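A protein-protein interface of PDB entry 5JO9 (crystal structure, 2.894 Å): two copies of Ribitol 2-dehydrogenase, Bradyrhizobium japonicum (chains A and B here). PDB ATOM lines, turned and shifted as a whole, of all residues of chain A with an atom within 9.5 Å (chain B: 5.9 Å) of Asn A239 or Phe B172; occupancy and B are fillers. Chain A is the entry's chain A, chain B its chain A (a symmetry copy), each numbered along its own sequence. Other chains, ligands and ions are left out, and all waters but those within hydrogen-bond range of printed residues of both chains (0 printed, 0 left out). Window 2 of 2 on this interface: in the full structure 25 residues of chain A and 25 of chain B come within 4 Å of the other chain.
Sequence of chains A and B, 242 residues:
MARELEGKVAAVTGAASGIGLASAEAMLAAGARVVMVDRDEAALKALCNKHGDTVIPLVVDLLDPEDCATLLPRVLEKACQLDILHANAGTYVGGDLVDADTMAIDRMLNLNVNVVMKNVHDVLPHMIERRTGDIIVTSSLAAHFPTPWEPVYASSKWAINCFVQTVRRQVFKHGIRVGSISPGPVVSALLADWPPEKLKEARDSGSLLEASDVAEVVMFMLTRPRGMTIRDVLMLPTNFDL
Among the printed residues, pairs that only touch across the chains: Thr A238 with Phe B172 (3.1 Å), Asp A241 with Phe B172 (3.1 Å), Leu A236 with Arg B168 (3.2 Å), Asn A239 with Phe B172 (3.6 Å), Thr A238 with Ile B176 (3.7 Å), Pro A237 with Arg B168 (3.8 Å) and Pro A237 with Gly B227 (3.8 Å).
The guanidinium group (NH2) of Arg B168 sits at hydrogen-bond distance from the backbone carbonyl oxygen (O) of Thr A238 (3.1 Å). The backbone carbonyl oxygen (O) of Gly B227 sits at hydrogen-bond distance from the side-chain hydroxyl (OG1) of Thr A238 (2.9 Å). The backbone carbonyl oxygen (O) of Phe A240 lies within hydrogen-bond range of the guanidinium group (NH2) of Arg B168 (3.2 Å). NH2 of Arg B169 is in salt-bridge range of OD2 of Asp A241 (2.8 Å). The chain-end carboxylate (OXT) of Leu A242 is in salt-bridge range of the guanidinium group (NH1) of Arg B168, 2.8 Å away. The backbone NH (N) of Leu A242 lies close to the guanidinium group (NE) of Arg B169 (3.4 Å).
The side-chain carboxylate (OE1) of Glu A201 sits at hydrogen-bond distance from the backbone NH (N) of Asp A241 (2.7 Å).
Printed residues of chain B within 4 Å of Phe A240: Arg B168 (3.2 Å). Phe B172 touches just these residues of chain A: Thr A238 (3.1 Å), Asn A239 (3.6 Å) and Asp A241 (3.1 Å). Of the printed residues of chain A, Gly B227 touches Pro A237 and Thr A238. The nearest residue of chain B that does not touch Asn A239 is Lys B173 (4.7 Å).
Hydrophobic or aromatic side chains of chain B within 4 Å of the printed part of chain A: Phe B172. Of the 19 printed residues of chain A, 7 touch a printed residue of chain B. Printed residues of chain A that touch a printed residue of chain B: Leu A236, Pro A237, Thr A238, Asn A239, Phe A240, Asp A241 and Leu A242. Hydrophobic or aromatic side chains of chain A within 4 Å of the printed part of chain B: Leu A236. Along chain A the printed residues that touch a printed residue of chain B span positions 236 to 242. Among the printed residues, Asp or Glu carboxylates within 4 Å of a Lys or Arg side-chain nitrogen of the other chain: Asp A241 with Arg B169 (2.8 Å).
No position is printed for both chains. Of the 13 pairs that touch across the chains among the printed residues, none has its exchanged pair printed and touching as well.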
ATOM      1  N   PRO A 185      -5.058 -19.072 -24.145  1.00  0.00           N
ATOM      2  CA  PRO A 185      -3.784 -19.784 -24.295  1.00  0.00           C
ATOM      3  C   PRO A 185      -3.635 -20.353 -25.696  1.00  0.00           C
ATOM      4  O   PRO A 185      -4.598 -20.825 -26.306  1.00  0.00           O
ATOM      5  CB  PRO A 185      -3.863 -20.895 -23.239  1.00  0.00           C
ATOM      6  CG  PRO A 185      -4.993 -20.501 -22.333  1.00  0.00           C
ATOM      7  CD  PRO A 185      -5.953 -19.766 -23.207  1.00  0.00           C
ATOM      8  N   LEU A 199      -2.891 -25.007 -16.631  1.00  0.00           N
ATOM      9  CA  LEU A 199      -2.084 -25.846 -17.507  1.00  0.00           C
ATOM     10  C   LEU A 199      -2.813 -27.179 -17.646  1.00  0.00           C
ATOM     11  O   LEU A 199      -3.275 -27.539 -18.733  1.00  0.00           O
ATOM     12  CB  LEU A 199      -0.679 -26.056 -16.931  1.00  0.00           C
ATOM     13  CG  LEU A 199       0.566 -25.938 -17.814  1.00  0.00           C
ATOM     14  CD1 LEU A 199       1.704 -26.742 -17.187  1.00  0.00           C
ATOM     15  CD2 LEU A 199       0.323 -26.407 -19.234  1.00  0.00           C
ATOM     16  N   LYS A 200      -2.912 -27.918 -16.537  1.00  0.00           N
ATOM     17  CA  LYS A 200      -3.872 -29.004 -16.383  1.00  0.00           C
ATOM     18  C   LYS A 200      -5.200 -28.683 -17.059  1.00  0.00           C
ATOM     19  O   LYS A 200      -5.837 -29.568 -17.639  1.00  0.00           O
ATOM     20  CB  LYS A 200      -4.106 -29.291 -14.898  1.00  0.00           C
ATOM     21  CG  LYS A 200      -3.045 -30.161 -14.244  1.00  0.00           C
ATOM     22  CD  LYS A 200      -3.686 -31.150 -13.285  1.00  0.00           C
ATOM     23  CE  LYS A 200      -2.834 -31.396 -12.057  1.00  0.00           C
ATOM     24  NZ  LYS A 200      -3.523 -32.323 -11.122  1.00  0.00           N
ATOM     25  N   GLU A 201      -5.643 -27.428 -16.964  1.00  0.00           N
ATOM     26  CA  GLU A 201      -6.782 -26.993 -17.763  1.00  0.00           C
ATOM     27  C   GLU A 201      -6.453 -27.070 -19.249  1.00  0.00           C
ATOM     28  O   GLU A 201      -7.250 -27.568 -20.050  1.00  0.00           O
ATOM     29  CB  GLU A 201      -7.185 -25.572 -17.370  1.00  0.00           C
ATOM     30  CG  GLU A 201      -8.029 -24.848 -18.411  1.00  0.00           C
ATOM     31  CD  GLU A 201      -9.371 -25.511 -18.659  1.00  0.00           C
ATOM     32  OE1 GLU A 201     -10.393 -24.954 -18.211  1.00  0.00           O
ATOM     33  OE2 GLU A 201      -9.409 -26.585 -19.295  1.00  0.00           O
ATOM     34  N   ALA A 202      -5.264 -26.597 -19.628  1.00  0.00           N
ATOM     35  CA  ALA A 202      -4.839 -26.560 -21.023  1.00  0.00           C
ATOM     36  C   ALA A 202      -4.690 -27.960 -21.607  1.00  0.00           C
ATOM     37  O   ALA A 202      -4.411 -28.108 -22.800  1.00  0.00           O
ATOM     38  CB  ALA A 202      -3.521 -25.789 -21.163  1.00  0.00           C
ATOM     39  N   ARG A 203      -4.873 -28.997 -20.788  1.00  0.00           N
ATOM     40  CA  ARG A 203      -4.978 -30.352 -21.340  1.00  0.00           C
ATOM     41  C   ARG A 203      -6.287 -30.593 -22.053  1.00  0.00           C
ATOM     42  O   ARG A 203      -6.576 -31.760 -22.346  1.00  0.00           O
ATOM     43  CB  ARG A 203      -4.814 -31.397 -20.236  1.00  0.00           C
ATOM     44  CG  ARG A 203      -3.501 -31.327 -19.491  1.00  0.00           C
ATOM     45  CD  ARG A 203      -3.583 -32.110 -18.193  1.00  0.00           C
ATOM     46  NE  ARG A 203      -2.372 -31.978 -17.388  1.00  0.00           N
ATOM     47  CZ  ARG A 203      -2.021 -32.808 -16.410  1.00  0.00           C
ATOM     48  NH1 ARG A 203      -2.782 -33.855 -16.113  1.00  0.00           N
ATOM     49  NH2 ARG A 203      -0.902 -32.598 -15.731  1.00  0.00           N
ATOM     50  N   ASP A 204      -7.066 -29.551 -22.332  1.00  0.00           N
ATOM     51  CA  ASP A 204      -8.352 -29.724 -22.989  1.00  0.00           C
ATOM     52  C   ASP A 204      -8.159 -30.420 -24.327  1.00  0.00           C
ATOM     53  O   ASP A 204      -7.478 -29.902 -25.215  1.00  0.00           O
ATOM     54  CB  ASP A 204      -9.038 -28.367 -23.186  1.00  0.00           C
ATOM     55  CG  ASP A 204      -8.070 -27.269 -23.612  1.00  0.00           C
ATOM     56  OD1 ASP A 204      -6.976 -27.183 -23.018  1.00  0.00           O
ATOM     57  OD2 ASP A 204      -8.405 -26.488 -24.529  1.00  0.00           O
ATOM     58  N   SER A 205      -8.749 -31.607 -24.471  1.00  0.00           N
ATOM     59  CA  SER A 205      -8.860 -32.199 -25.797  1.00  0.00           C
ATOM     60  C   SER A 205      -9.499 -31.258 -26.815  1.00  0.00           C
ATOM     61  O   SER A 205      -9.470 -31.560 -28.015  1.00  0.00           O
ATOM     62  CB  SER A 205      -9.646 -33.502 -25.700  1.00  0.00           C
ATOM     63  OG  SER A 205      -8.861 -34.504 -25.073  1.00  0.00           O
ATOM     64  N   GLY A 206     -10.097 -30.153 -26.369  1.00  0.00           N
ATOM     65  CA  GLY A 206     -10.379 -29.016 -27.225  1.00  0.00           C
ATOM     66  C   GLY A 206      -9.097 -28.309 -27.620  1.00  0.00           C
ATOM     67  O   GLY A 206      -8.874 -27.142 -27.280  1.00  0.00           O
ATOM     68  N   SER A 207      -8.244 -29.049 -28.329  1.00  0.00           N
ATOM     69  CA  SER A 207      -6.906 -28.674 -28.786  1.00  0.00           C
ATOM     70  C   SER A 207      -6.467 -27.226 -28.597  1.00  0.00           C
ATOM     71  O   SER A 207      -5.829 -26.674 -29.498  1.00  0.00           O
ATOM     72  CB  SER A 207      -6.792 -29.015 -30.277  1.00  0.00           C
ATOM     73  OG  SER A 207      -5.816 -28.215 -30.941  1.00  0.00           O
ATOM     74  N   LEU A 208      -6.730 -26.616 -27.451  1.00  0.00           N
ATOM     75  CA  LEU A 208      -6.182 -25.281 -27.179  1.00  0.00           C
ATOM     76  C   LEU A 208      -6.506 -24.373 -28.370  1.00  0.00           C
ATOM     77  O   LEU A 208      -7.504 -24.567 -29.071  1.00  0.00           O
ATOM     78  CB  LEU A 208      -4.689 -25.425 -26.851  1.00  0.00           C
ATOM     79  CG  LEU A 208      -4.182 -25.508 -25.404  1.00  0.00           C
ATOM     80  CD1 LEU A 208      -2.948 -24.628 -25.287  1.00  0.00           C
ATOM     81  CD2 LEU A 208      -5.232 -25.103 -24.389  1.00  0.00           C
ATOM     82  N   LEU A 209      -5.677 -23.359 -28.596  1.00  0.00           N
ATOM     83  CA  LEU A 209      -5.779 -22.464 -29.741  1.00  0.00           C
ATOM     84  C   LEU A 209      -4.534 -22.603 -30.603  1.00  0.00           C
ATOM     85  O   LEU A 209      -3.411 -22.608 -30.091  1.00  0.00           O
ATOM     86  CB  LEU A 209      -5.915 -21.019 -29.287  1.00  0.00           C
ATOM     87  CG  LEU A 209      -6.916 -20.207 -30.094  1.00  0.00           C
ATOM     88  CD1 LEU A 209      -7.407 -19.028 -29.286  1.00  0.00           C
ATOM     89  CD2 LEU A 209      -6.273 -19.756 -31.395  1.00  0.00           C
ATOM     90  N   LEU A 236     -10.772 -17.290 -27.400  1.00  0.00           N
ATOM     91  CA  LEU A 236     -10.211 -18.258 -26.469  1.00  0.00           C
ATOM     92  C   LEU A 236     -10.598 -19.652 -26.935  1.00  0.00           C
ATOM     93  O   LEU A 236     -11.588 -19.814 -27.658  1.00  0.00           O
ATOM     94  CB  LEU A 236     -10.702 -18.016 -25.033  1.00  0.00           C
ATOM     95  CG  LEU A 236     -12.144 -17.536 -24.816  1.00  0.00           C
ATOM     96  CD1 LEU A 236     -13.158 -18.358 -25.600  1.00  0.00           C
ATOM     97  CD2 LEU A 236     -12.479 -17.572 -23.332  1.00  0.00           C
ATOM     98  N   PRO A 237      -9.831 -20.675 -26.560  1.00  0.00           N
ATOM     99  CA  PRO A 237     -10.258 -22.048 -26.850  1.00  0.00           C
ATOM    100  C   PRO A 237     -11.606 -22.336 -26.211  1.00  0.00           C
ATOM    101  O   PRO A 237     -11.830 -22.049 -25.032  1.00  0.00           O
ATOM    102  CB  PRO A 237      -9.138 -22.903 -26.244  1.00  0.00           C
ATOM    103  CG  PRO A 237      -7.952 -22.008 -26.255  1.00  0.00           C
ATOM    104  CD  PRO A 237      -8.497 -20.647 -25.937  1.00  0.00           C
ATOM    105  N   THR A 238     -12.512 -22.905 -27.009  1.00  0.00           N
ATOM    106  CA  THR A 238     -13.872 -23.138 -26.533  1.00  0.00           C
ATOM    107  C   THR A 238     -13.873 -23.943 -25.239  1.00  0.00           C
ATOM    108  O   THR A 238     -14.704 -23.709 -24.355  1.00  0.00           O
ATOM    109  CB  THR A 238     -14.687 -23.853 -27.611  1.00  0.00           C
ATOM    110  OG1 THR A 238     -14.563 -23.150 -28.854  1.00  0.00           O
ATOM    111  CG2 THR A 238     -16.157 -23.921 -27.215  1.00  0.00           C
ATOM    112  N   ASN A 239     -12.944 -24.887 -25.105  1.00  0.00           N
ATOM    113  CA  ASN A 239     -12.872 -25.760 -23.936  1.00  0.00           C
ATOM    114  C   ASN A 239     -11.841 -25.276 -22.925  1.00  0.00           C
ATOM    115  O   ASN A 239     -11.141 -26.079 -22.304  1.00  0.00           O
ATOM    116  CB  ASN A 239     -12.571 -27.189 -24.372  1.00  0.00           C
ATOM    117  CG  ASN A 239     -13.721 -27.816 -25.133  1.00  0.00           C
ATOM    118  OD1 ASN A 239     -13.808 -27.699 -26.355  1.00  0.00           O
ATOM    119  ND2 ASN A 239     -14.618 -28.478 -24.410  1.00  0.00           N
ATOM    120  N   PHE A 240     -11.731 -23.963 -22.746  1.00  0.00           N
ATOM    121  CA  PHE A 240     -10.859 -23.365 -21.745  1.00  0.00           C
ATOM    122  C   PHE A 240     -11.718 -22.583 -20.762  1.00  0.00           C
ATOM    123  O   PHE A 240     -12.515 -21.732 -21.169  1.00  0.00           O
ATOM    124  CB  PHE A 240      -9.816 -22.456 -22.402  1.00  0.00           C
ATOM    125  CG  PHE A 240      -8.815 -21.887 -21.442  1.00  0.00           C
ATOM    126  CD1 PHE A 240      -7.906 -22.709 -20.806  1.00  0.00           C
ATOM    127  CD2 PHE A 240      -8.772 -20.528 -21.188  1.00  0.00           C
ATOM    128  CE1 PHE A 240      -6.980 -22.192 -19.923  1.00  0.00           C
ATOM    129  CE2 PHE A 240      -7.846 -20.004 -20.307  1.00  0.00           C
ATOM    130  CZ  PHE A 240      -6.949 -20.839 -19.674  1.00  0.00           C
ATOM    131  N   ASP A 241     -11.560 -22.880 -19.472  1.00  0.00           N
ATOM    132  CA  ASP A 241     -12.438 -22.348 -18.430  1.00  0.00           C
ATOM    133  C   ASP A 241     -11.892 -21.006 -17.956  1.00  0.00           C
ATOM    134  O   ASP A 241     -10.986 -20.951 -17.121  1.00  0.00           O
ATOM    135  CB  ASP A 241     -12.550 -23.337 -17.275  1.00  0.00           C
ATOM    136  CG  ASP A 241     -13.746 -23.068 -16.386  1.00  0.00           C
ATOM    137  OD1 ASP A 241     -14.860 -22.886 -16.922  1.00  0.00           O
ATOM    138  OD2 ASP A 241     -13.572 -23.041 -15.150  1.00  0.00           O
ATOM    139  N   LEU A 242     -12.447 -19.919 -18.488  1.00  0.00           N
ATOM    140  CA  LEU A 242     -12.113 -18.572 -18.026  1.00  0.00           C
ATOM    141  C   LEU A 242     -13.026 -17.539 -18.680  1.00  0.00           C
ATOM    142  O   LEU A 242     -13.195 -16.428 -18.171  1.00  0.00           O
ATOM    143  CB  LEU A 242     -10.651 -18.229 -18.325  1.00  0.00           C
ATOM    144  CG  LEU A 242     -10.044 -17.204 -17.362  1.00  0.00           C
ATOM    145  CD1 LEU A 242      -9.412 -17.910 -16.176  1.00  0.00           C
ATOM    146  CD2 LEU A 242      -9.033 -16.306 -18.057  1.00  0.00           C
ATOM    147  OXT LEU A 242     -13.613 -17.788 -19.734  1.00  0.00           O
ATOM    148  N   VAL B 167     -21.601 -16.604 -18.510  1.00  0.00           N
ATOM    149  CA  VAL B 167     -22.516 -17.701 -18.817  1.00  0.00           C
ATOM    150  C   VAL B 167     -21.822 -18.752 -19.671  1.00  0.00           C
ATOM    151  O   VAL B 167     -22.072 -19.953 -19.520  1.00  0.00           O
ATOM    152  CB  VAL B 167     -23.791 -17.172 -19.503  1.00  0.00           C
ATOM    153  CG1 VAL B 167     -23.483 -16.630 -20.890  1.00  0.00           C
ATOM    154  CG2 VAL B 167     -24.839 -18.274 -19.588  1.00  0.00           C
ATOM    155  N   ARG B 168     -20.947 -18.326 -20.584  1.00  0.00           N
ATOM    156  CA  ARG B 168     -20.274 -19.291 -21.444  1.00  0.00           C
ATOM    157  C   ARG B 168     -19.358 -20.214 -20.655  1.00  0.00           C
ATOM    158  O   ARG B 168     -19.061 -21.317 -21.120  1.00  0.00           O
ATOM    159  CB  ARG B 168     -19.483 -18.572 -22.546  1.00  0.00           C
ATOM    160  CG  ARG B 168     -18.088 -18.071 -22.166  1.00  0.00           C
ATOM    161  CD  ARG B 168     -17.191 -17.989 -23.391  1.00  0.00           C
ATOM    162  NE  ARG B 168     -16.489 -19.248 -23.633  1.00  0.00           N
ATOM    163  CZ  ARG B 168     -15.461 -19.682 -22.909  1.00  0.00           C
ATOM    164  NH1 ARG B 168     -15.015 -18.963 -21.887  1.00  0.00           N
ATOM    165  NH2 ARG B 168     -14.882 -20.839 -23.200  1.00  0.00           N
ATOM    166  N   ARG B 169     -18.904 -19.787 -19.475  1.00  0.00           N
ATOM    167  CA  ARG B 169     -18.032 -20.626 -18.662  1.00  0.00           C
ATOM    168  C   ARG B 169     -18.751 -21.849 -18.110  1.00  0.00           C
ATOM    169  O   ARG B 169     -18.088 -22.813 -17.713  1.00  0.00           O
ATOM    170  CB  ARG B 169     -17.444 -19.818 -17.505  1.00  0.00           C
ATOM    171  CG  ARG B 169     -16.148 -19.099 -17.836  1.00  0.00           C
ATOM    172  CD  ARG B 169     -15.470 -18.584 -16.575  1.00  0.00           C
ATOM    173  NE  ARG B 169     -14.636 -19.603 -15.943  1.00  0.00           N
ATOM    174  CZ  ARG B 169     -13.964 -19.425 -14.810  1.00  0.00           C
ATOM    175  NH1 ARG B 169     -14.024 -18.265 -14.169  1.00  0.00           N
ATOM    176  NH2 ARG B 169     -13.230 -20.411 -14.315  1.00  0.00           N
ATOM    177  N   GLN B 170     -20.084 -21.833 -18.073  1.00  0.00           N
ATOM    178  CA  GLN B 170     -20.865 -22.933 -17.522  1.00  0.00           C
ATOM    179  C   GLN B 170     -21.681 -23.652 -18.589  1.00  0.00           C
ATOM    180  O   GLN B 170     -22.677 -24.310 -18.266  1.00  0.00           O
ATOM    181  CB  GLN B 170     -21.777 -22.420 -16.406  1.00  0.00           C
ATOM    182  CG  GLN B 170     -22.644 -21.237 -16.801  1.00  0.00           C
ATOM    183  CD  GLN B 170     -23.405 -20.656 -15.629  1.00  0.00           C
ATOM    184  OE1 GLN B 170     -22.844 -20.433 -14.556  1.00  0.00           O
ATOM    185  NE2 GLN B 170     -24.687 -20.402 -15.827  1.00  0.00           N
ATOM    186  N   VAL B 171     -21.278 -23.544 -19.854  1.00  0.00           N
ATOM    187  CA  VAL B 171     -22.028 -24.147 -20.950  1.00  0.00           C
ATOM    188  C   VAL B 171     -21.083 -24.735 -21.992  1.00  0.00           C
ATOM    189  O   VAL B 171     -21.464 -25.635 -22.748  1.00  0.00           O
ATOM    190  CB  VAL B 171     -22.974 -23.117 -21.594  1.00  0.00           C
ATOM    191  CG1 VAL B 171     -23.744 -23.739 -22.743  1.00  0.00           C
ATOM    192  CG2 VAL B 171     -23.937 -22.562 -20.564  1.00  0.00           C
ATOM    193  N   PHE B 172     -19.844 -24.239 -22.045  1.00  0.00           N
ATOM    194  CA  PHE B 172     -18.942 -24.642 -23.119  1.00  0.00           C
ATOM    195  C   PHE B 172     -18.647 -26.137 -23.102  1.00  0.00           C
ATOM    196  O   PHE B 172     -18.242 -26.686 -24.133  1.00  0.00           O
ATOM    197  CB  PHE B 172     -17.636 -23.846 -23.047  1.00  0.00           C
ATOM    198  CG  PHE B 172     -16.773 -24.186 -21.866  1.00  0.00           C
ATOM    199  CD1 PHE B 172     -15.836 -25.201 -21.944  1.00  0.00           C
ATOM    200  CD2 PHE B 172     -16.885 -23.478 -20.682  1.00  0.00           C
ATOM    201  CE1 PHE B 172     -15.037 -25.510 -20.863  1.00  0.00           C
ATOM    202  CE2 PHE B 172     -16.088 -23.783 -19.598  1.00  0.00           C
ATOM    203  CZ  PHE B 172     -15.163 -24.799 -19.688  1.00  0.00           C
ATOM    204  N   LYS B 173     -18.844 -26.812 -21.965  1.00  0.00           N
ATOM    205  CA  LYS B 173     -18.632 -28.254 -21.915  1.00  0.00           C
ATOM    206  C   LYS B 173     -19.652 -29.022 -22.744  1.00  0.00           C
ATOM    207  O   LYS B 173     -19.471 -30.226 -22.954  1.00  0.00           O
ATOM    208  CB  LYS B 173     -18.672 -28.754 -20.468  1.00  0.00           C
ATOM    209  CG  LYS B 173     -20.078 -28.964 -19.897  1.00  0.00           C
ATOM    210  CD  LYS B 173     -20.049 -29.322 -18.414  1.00  0.00           C
ATOM    211  CE  LYS B 173     -19.230 -30.583 -18.145  1.00  0.00           C
ATOM    212  NZ  LYS B 173     -19.232 -30.969 -16.707  1.00  0.00           N
ATOM    213  N   HIS B 174     -20.709 -28.361 -23.217  1.00  0.00           N
ATOM    214  CA  HIS B 174     -21.753 -29.002 -24.005  1.00  0.00           C
ATOM    215  C   HIS B 174     -21.661 -28.642 -25.485  1.00  0.00           C
ATOM    216  O   HIS B 174     -22.652 -28.766 -26.212  1.00  0.00           O
ATOM    217  CB  HIS B 174     -23.125 -28.630 -23.446  1.00  0.00           C
ATOM    218  CG  HIS B 174     -23.317 -29.030 -22.016  1.00  0.00           C
ATOM    219  ND1 HIS B 174     -23.878 -28.191 -21.076  1.00  0.00           N
ATOM    220  CD2 HIS B 174     -23.032 -30.183 -21.367  1.00  0.00           C
ATOM    221  CE1 HIS B 174     -23.924 -28.809 -19.910  1.00  0.00           C
ATOM    222  NE2 HIS B 174     -23.416 -30.019 -20.059  1.00  0.00           N
ATOM    223  N   GLY B 175     -20.493 -28.202 -25.943  1.00  0.00           N
ATOM    224  CA  GLY B 175     -20.300 -27.873 -27.346  1.00  0.00           C
ATOM    225  C   GLY B 175     -21.019 -26.616 -27.792  1.00  0.00           C
ATOM    226  O   GLY B 175     -21.625 -26.605 -28.872  1.00  0.00           O
ATOM    227  N   ILE B 176     -20.958 -25.552 -26.996  1.00  0.00           N
ATOM    228  CA  ILE B 176     -21.677 -24.319 -27.283  1.00  0.00           C
ATOM    229  C   ILE B 176     -20.689 -23.161 -27.306  1.00  0.00           C
ATOM    230  O   ILE B 176     -19.694 -23.149 -26.575  1.00  0.00           O
ATOM    231  CB  ILE B 176     -22.793 -24.065 -26.247  1.00  0.00           C
ATOM    232  CG1 ILE B 176     -23.676 -25.316 -26.139  1.00  0.00           C
ATOM    233  CG2 ILE B 176     -23.588 -22.807 -26.610  1.00  0.00           C
ATOM    234  CD1 ILE B 176     -25.098 -25.076 -25.666  1.00  0.00           C
ATOM    235  N   GLY B 227     -13.611 -25.321 -32.546  1.00  0.00           N
ATOM    236  CA  GLY B 227     -12.676 -25.306 -31.436  1.00  0.00           C
ATOM    237  C   GLY B 227     -12.400 -23.924 -30.887  1.00  0.00           C
ATOM    238  O   GLY B 227     -11.926 -23.803 -29.752  1.00  0.00           O
